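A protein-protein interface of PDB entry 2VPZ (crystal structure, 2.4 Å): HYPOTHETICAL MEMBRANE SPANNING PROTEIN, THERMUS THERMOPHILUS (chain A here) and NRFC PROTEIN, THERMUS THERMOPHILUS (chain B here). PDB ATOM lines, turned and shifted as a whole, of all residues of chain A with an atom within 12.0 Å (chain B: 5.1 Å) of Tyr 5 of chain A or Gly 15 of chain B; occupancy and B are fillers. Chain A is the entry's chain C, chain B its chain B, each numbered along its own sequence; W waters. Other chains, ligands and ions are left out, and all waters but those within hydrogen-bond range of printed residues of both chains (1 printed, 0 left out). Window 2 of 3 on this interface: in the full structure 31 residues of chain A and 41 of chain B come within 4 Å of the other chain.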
ATOM      1  N   ALA A   2     -15.986  -3.175 -15.709  1.00  0.00           N
ATOM      2  CA  ALA A   2     -17.068  -2.250 -15.270  1.00  0.00           C
ATOM      3  C   ALA A   2     -16.642  -0.779 -15.582  1.00  0.00           C
ATOM      4  O   ALA A   2     -17.416  -0.054 -16.208  1.00  0.00           O
ATOM      5  CB  ALA A   2     -17.375  -2.489 -13.768  1.00  0.00           C
ATOM      6  N   GLU A   3     -15.426  -0.360 -15.182  1.00  0.00           N
ATOM      7  CA  GLU A   3     -14.830   0.995 -15.464  1.00  0.00           C
ATOM      8  C   GLU A   3     -13.696   0.910 -16.526  1.00  0.00           C
ATOM      9  O   GLU A   3     -12.944  -0.065 -16.513  1.00  0.00           O
ATOM     10  CB  GLU A   3     -14.155   1.618 -14.236  1.00  0.00           C
ATOM     11  CG  GLU A   3     -14.972   1.644 -12.989  1.00  0.00           C
ATOM     12  CD  GLU A   3     -16.067   2.678 -13.039  1.00  0.00           C
ATOM     13  OE1 GLU A   3     -15.751   3.866 -12.833  1.00  0.00           O
ATOM     14  OE2 GLU A   3     -17.230   2.301 -13.301  1.00  0.00           O
ATOM     15  N   PHE A   4     -13.541   1.913 -17.395  1.00  0.00           N
ATOM     16  CA  PHE A   4     -12.462   1.920 -18.411  1.00  0.00           C
ATOM     17  C   PHE A   4     -11.618   3.210 -18.458  1.00  0.00           C
ATOM     18  O   PHE A   4     -12.019   4.228 -17.909  1.00  0.00           O
ATOM     19  CB  PHE A   4     -12.995   1.786 -19.866  1.00  0.00           C
ATOM     20  CG  PHE A   4     -13.879   0.598 -20.129  1.00  0.00           C
ATOM     21  CD1 PHE A   4     -15.254   0.679 -19.920  1.00  0.00           C
ATOM     22  CD2 PHE A   4     -13.328  -0.607 -20.565  1.00  0.00           C
ATOM     23  CE1 PHE A   4     -16.086  -0.434 -20.142  1.00  0.00           C
ATOM     24  CE2 PHE A   4     -14.135  -1.732 -20.794  1.00  0.00           C
ATOM     25  CZ  PHE A   4     -15.518  -1.649 -20.577  1.00  0.00           C
ATOM     26  N   TYR A   5     -10.439   3.121 -19.097  1.00  0.00           N
ATOM     27  CA  TYR A   5      -9.606   4.288 -19.442  1.00  0.00           C
ATOM     28  C   TYR A   5      -9.564   4.078 -20.954  1.00  0.00           C
ATOM     29  O   TYR A   5      -9.019   3.082 -21.482  1.00  0.00           O
ATOM     30  CB  TYR A   5      -8.229   4.352 -18.804  1.00  0.00           C
ATOM     31  CG  TYR A   5      -8.329   4.780 -17.362  1.00  0.00           C
ATOM     32  CD1 TYR A   5      -7.897   3.927 -16.352  1.00  0.00           C
ATOM     33  CD2 TYR A   5      -8.902   6.002 -16.997  1.00  0.00           C
ATOM     34  CE1 TYR A   5      -8.029   4.258 -15.017  1.00  0.00           C
ATOM     35  CE2 TYR A   5      -9.045   6.363 -15.645  1.00  0.00           C
ATOM     36  CZ  TYR A   5      -8.600   5.474 -14.654  1.00  0.00           C
ATOM     37  OH  TYR A   5      -8.712   5.780 -13.315  1.00  0.00           O
ATOM     38  N   GLY A   6     -10.215   5.023 -21.622  1.00  0.00           N
ATOM     39  CA  GLY A   6     -10.434   4.920 -23.035  1.00  0.00           C
ATOM     40  C   GLY A   6     -11.692   4.042 -23.048  1.00  0.00           C
ATOM     41  O   GLY A   6     -12.413   3.970 -22.039  1.00  0.00           O
ATOM     42  N   LEU A   7     -11.920   3.342 -24.158  1.00  0.00           N
ATOM     43  CA  LEU A   7     -13.079   2.458 -24.401  1.00  0.00           C
ATOM     44  C   LEU A   7     -12.810   1.344 -25.437  1.00  0.00           C
ATOM     45  O   LEU A   7     -11.968   1.541 -26.317  1.00  0.00           O
ATOM     46  CB  LEU A   7     -14.247   3.253 -24.996  1.00  0.00           C
ATOM     47  CG  LEU A   7     -15.042   4.281 -24.199  1.00  0.00           C
ATOM     48  CD1 LEU A   7     -15.869   5.194 -25.150  1.00  0.00           C
ATOM     49  CD2 LEU A   7     -15.915   3.518 -23.172  1.00  0.00           C
ATOM     50  N   PRO A   8     -13.478   0.157 -25.314  1.00  0.00           N
ATOM     51  CA  PRO A   8     -13.282  -0.911 -26.314  1.00  0.00           C
ATOM     52  C   PRO A   8     -14.100  -0.421 -27.520  1.00  0.00           C
ATOM     53  O   PRO A   8     -15.040   0.358 -27.327  1.00  0.00           O
ATOM     54  CB  PRO A   8     -13.963  -2.153 -25.720  1.00  0.00           C
ATOM     55  CG  PRO A   8     -14.724  -1.684 -24.530  1.00  0.00           C
ATOM     56  CD  PRO A   8     -14.055  -0.387 -24.079  1.00  0.00           C
ATOM     57  N   ASN A   9     -13.761  -0.870 -28.726  1.00  0.00           N
ATOM     58  CA  ASN A   9     -14.466  -0.505 -29.958  1.00  0.00           C
ATOM     59  C   ASN A   9     -15.675  -1.447 -30.157  1.00  0.00           C
ATOM     60  O   ASN A   9     -15.671  -2.300 -31.046  1.00  0.00           O
ATOM     61  CB  ASN A   9     -13.503  -0.605 -31.145  1.00  0.00           C
ATOM     62  CG  ASN A   9     -12.247   0.238 -30.956  1.00  0.00           C
ATOM     63  OD1 ASN A   9     -11.140  -0.287 -30.822  1.00  0.00           O
ATOM     64  ND2 ASN A   9     -12.422   1.549 -30.931  1.00  0.00           N
ATOM     65  N   ALA A  10     -16.703  -1.293 -29.317  1.00  0.00           N
ATOM     66  CA  ALA A  10     -17.896  -2.132 -29.327  1.00  0.00           C
ATOM     67  C   ALA A  10     -19.169  -1.492 -29.880  1.00  0.00           C
ATOM     68  O   ALA A  10     -20.277  -1.944 -29.577  1.00  0.00           O
ATOM     69  CB  ALA A  10     -18.176  -2.669 -27.898  1.00  0.00           C
ATOM     70  N   CYS B  13       0.304  -4.727 -12.586  1.00  0.00           N
ATOM     71  CA  CYS B  13      -0.473  -3.688 -13.290  1.00  0.00           C
ATOM     72  C   CYS B  13      -1.355  -2.820 -12.342  1.00  0.00           C
ATOM     73  O   CYS B  13      -2.099  -3.348 -11.509  1.00  0.00           O
ATOM     74  CB  CYS B  13      -1.322  -4.284 -14.443  1.00  0.00           C
ATOM     75  SG  CYS B  13      -1.890  -2.969 -15.660  1.00  0.00           S
ATOM     76  N   VAL B  14      -1.266  -1.497 -12.449  1.00  0.00           N
ATOM     77  CA  VAL B  14      -2.055  -0.629 -11.574  1.00  0.00           C
ATOM     78  C   VAL B  14      -3.101   0.219 -12.300  1.00  0.00           C
ATOM     79  O   VAL B  14      -3.768   1.051 -11.686  1.00  0.00           O
ATOM     80  CB  VAL B  14      -1.127   0.254 -10.625  1.00  0.00           C
ATOM     81  CG1 VAL B  14      -0.140  -0.659  -9.870  1.00  0.00           C
ATOM     82  CG2 VAL B  14      -0.403   1.351 -11.411  1.00  0.00           C
ATOM     83  N   GLY B  15      -3.242  -0.036 -13.600  1.00  0.00           N
ATOM     84  CA  GLY B  15      -4.207   0.636 -14.458  1.00  0.00           C
ATOM     85  C   GLY B  15      -4.106   2.141 -14.667  1.00  0.00           C
ATOM     86  O   GLY B  15      -5.140   2.809 -14.769  1.00  0.00           O
ATOM     87  N   CYS B  16      -2.878   2.667 -14.703  1.00  0.00           N
ATOM     88  CA  CYS B  16      -2.529   4.092 -14.937  1.00  0.00           C
ATOM     89  C   CYS B  16      -2.479   4.037 -16.475  1.00  0.00           C
ATOM     90  O   CYS B  16      -1.494   3.583 -17.005  1.00  0.00           O
ATOM     91  CB  CYS B  16      -1.101   4.341 -14.424  1.00  0.00           C
ATOM     92  SG  CYS B  16       0.185   3.207 -15.415  1.00  0.00           S
ATOM     93  N   ALA B  17      -3.440   4.492 -17.248  1.00  0.00           N
ATOM     94  CA  ALA B  17      -3.246   4.191 -18.682  1.00  0.00           C
ATOM     95  C   ALA B  17      -1.954   4.685 -19.426  1.00  0.00           C
ATOM     96  O   ALA B  17      -2.060   5.187 -20.536  1.00  0.00           O
ATOM     97  CB  ALA B  17      -4.524   4.594 -19.469  1.00  0.00           C
ATOM     98  N   LEU B  36      -5.740   0.372 -27.786  1.00  0.00           N
ATOM     99  CA  LEU B  36      -5.463  -0.093 -26.389  1.00  0.00           C
ATOM    100  C   LEU B  36      -6.304   0.686 -25.355  1.00  0.00           C
ATOM    101  O   LEU B  36      -6.417   1.910 -25.478  1.00  0.00           O
ATOM    102  CB  LEU B  36      -3.944   0.108 -26.067  1.00  0.00           C
ATOM    103  CG  LEU B  36      -3.276  -0.058 -24.675  1.00  0.00           C
ATOM    104  CD1 LEU B  36      -3.874  -1.278 -24.006  1.00  0.00           C
ATOM    105  CD2 LEU B  36      -1.713  -0.201 -24.737  1.00  0.00           C
ATOM    106  N   TRP B  37      -6.903  -0.005 -24.384  1.00  0.00           N
ATOM    107  CA  TRP B  37      -7.732   0.581 -23.318  1.00  0.00           C
ATOM    108  C   TRP B  37      -7.508  -0.287 -22.091  1.00  0.00           C
ATOM    109  O   TRP B  37      -6.969  -1.384 -22.209  1.00  0.00           O
ATOM    110  CB  TRP B  37      -9.231   0.574 -23.673  1.00  0.00           C
ATOM    111  CG  TRP B  37      -9.818  -0.809 -24.043  1.00  0.00           C
ATOM    112  CD1 TRP B  37     -10.530  -1.687 -23.228  1.00  0.00           C
ATOM    113  CD2 TRP B  37      -9.751  -1.437 -25.332  1.00  0.00           C
ATOM    114  NE1 TRP B  37     -10.899  -2.808 -23.959  1.00  0.00           N
ATOM    115  CE2 TRP B  37     -10.431  -2.682 -25.243  1.00  0.00           C
ATOM    116  CE3 TRP B  37      -9.170  -1.067 -26.552  1.00  0.00           C
ATOM    117  CZ2 TRP B  37     -10.556  -3.555 -26.347  1.00  0.00           C
ATOM    118  CZ3 TRP B  37      -9.291  -1.928 -27.656  1.00  0.00           C
ATOM    119  CH2 TRP B  37      -9.981  -3.166 -27.537  1.00  0.00           C
ATOM    120  N   ILE B  38      -7.926   0.196 -20.928  1.00  0.00           N
ATOM    121  CA  ILE B  38      -7.776  -0.519 -19.667  1.00  0.00           C
ATOM    122  C   ILE B  38      -9.176  -0.780 -19.076  1.00  0.00           C
ATOM    123  O   ILE B  38      -9.995   0.136 -19.011  1.00  0.00           O
ATOM    124  CB  ILE B  38      -7.011   0.347 -18.552  1.00  0.00           C
ATOM    125  CG1 ILE B  38      -5.784   1.078 -19.130  1.00  0.00           C
ATOM    126  CG2 ILE B  38      -6.735  -0.541 -17.296  1.00  0.00           C
ATOM    127  CD1 ILE B  38      -4.657   0.233 -19.687  1.00  0.00           C
ATOM    128  N   GLU B  40     -11.270  -2.084 -15.565  1.00  0.00           N
ATOM    129  CA  GLU B  40     -11.019  -2.246 -14.121  1.00  0.00           C
ATOM    130  C   GLU B  40     -12.307  -2.776 -13.493  1.00  0.00           C
ATOM    131  O   GLU B  40     -13.376  -2.183 -13.676  1.00  0.00           O
ATOM    132  CB  GLU B  40     -10.570  -0.906 -13.461  1.00  0.00           C
ATOM    133  CG  GLU B  40     -10.729  -0.757 -11.893  1.00  0.00           C
ATOM    134  CD  GLU B  40     -10.034   0.514 -11.262  1.00  0.00           C
ATOM    135  OE1 GLU B  40      -9.266   1.224 -11.956  1.00  0.00           O
ATOM    136  OE2 GLU B  40     -10.258   0.784 -10.056  1.00  0.00           O
ATOM    137  N   PHE B  53      -7.101  -4.962 -12.822  1.00  0.00           N
ATOM    138  CA  PHE B  53      -6.759  -3.896 -13.771  1.00  0.00           C
ATOM    139  C   PHE B  53      -6.328  -4.669 -15.038  1.00  0.00           C
ATOM    140  O   PHE B  53      -5.435  -5.499 -14.958  1.00  0.00           O
ATOM    141  CB  PHE B  53      -5.595  -3.071 -13.224  1.00  0.00           C
ATOM    142  CG  PHE B  53      -5.851  -2.480 -11.868  1.00  0.00           C
ATOM    143  CD1 PHE B  53      -5.350  -3.089 -10.711  1.00  0.00           C
ATOM    144  CD2 PHE B  53      -6.600  -1.308 -11.751  1.00  0.00           C
ATOM    145  CE1 PHE B  53      -5.590  -2.529  -9.434  1.00  0.00           C
ATOM    146  CE2 PHE B  53      -6.857  -0.730 -10.505  1.00  0.00           C
ATOM    147  CZ  PHE B  53      -6.353  -1.337  -9.336  1.00  0.00           C
HETATM  148  O   HOH W   1      -7.715   3.863 -11.462  1.00  0.00           O
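Water W1 lies within hydrogen-bond range of OH of Tyr 5 of chain A and OE1 of Glu 40 of chain B.
O of Ile 38 of chain B lies within hydrogen-bond range of N of Tyr 5 of chain A (3.0 Å). O of Glu 40 of chain B is in hydrogen-bond range of N of Ala 2 of chain A, 3.5 Å away. The backbone NH (N) of Glu 40 of chain B is in hydrogen-bond range of the backbone carbonyl oxygen (O) of Glu 3 of chain A, 2.8 Å away.
Hydrophobic or aromatic side chains of chain A that line the printed part of chain B: Phe 4, Tyr 5 and Pro 8. Hydrophobic or aromatic side chains of chain B within 4 Å of the printed part of chain A: Ala 17 and Trp 37. Among the printed residues, 10 pairs touch across the chains. Among the printed residues, no Asp or Glu carboxylate lies within 4 Å of a Lys or Arg side-chain nitrogen of the other chain.
Among the printed residues, pairs that only touch across the chains: Glu 3 of chain A with Ile 38 of chain B, Phe 4 of chain A with Ile 38 of chain B, Tyr 5 of chain A with Gly 15 of chain B, Tyr 5 of chain A with Ala 17 of chain B, Tyr 5 of chain A with Trp 37 of chain B, Leu 7 of chain A with Trp 37 of chain B and Pro 8 of chain A with Trp 37 of chain B.
Of the printed residues of chain B, Tyr 5 of chain A touches Gly 15, Ala 17, Trp 37 and Ile 38. Gly 15 of chain B touches one residue of chain A. No residue of chain A comes within 4 Å of Cys 13 of chain B. No residue of chain A comes within 4 Å of Cys 16 of chain B. Of chain A, only Tyr 5 (3.8 Å) comes within 4 Å of Ala 17 of chain B. No residue of chain A comes within 4 Å of Phe 53 of chain B. Of the printed residues of chain A, Glu 40 of chain B touches Ala 2 (3.5 Å) and Glu 3 (2.8 Å). Of the printed residues of chain A, Trp 37 of chain B touches Tyr 5, Leu 7 and Pro 8. Of the printed residues of chain B, Glu 3 of chain A touches Ile 38 and Glu 40. Of the printed residues of chain B, Phe 4 of chain A touches Ile 38 (3.1 Å). Leu 36 of chain B touches none of the printed residues of chain A. Gly 6 of chain A touches none of the printed residues of chain B. The nearest residue of chain B that does not touch Tyr 5 of chain A is Glu 40 of chain B (4.5 Å). The nearest residue of chain A that does not touch Gly 15 of chain B is Phe 4 of chain A (7.5 Å).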
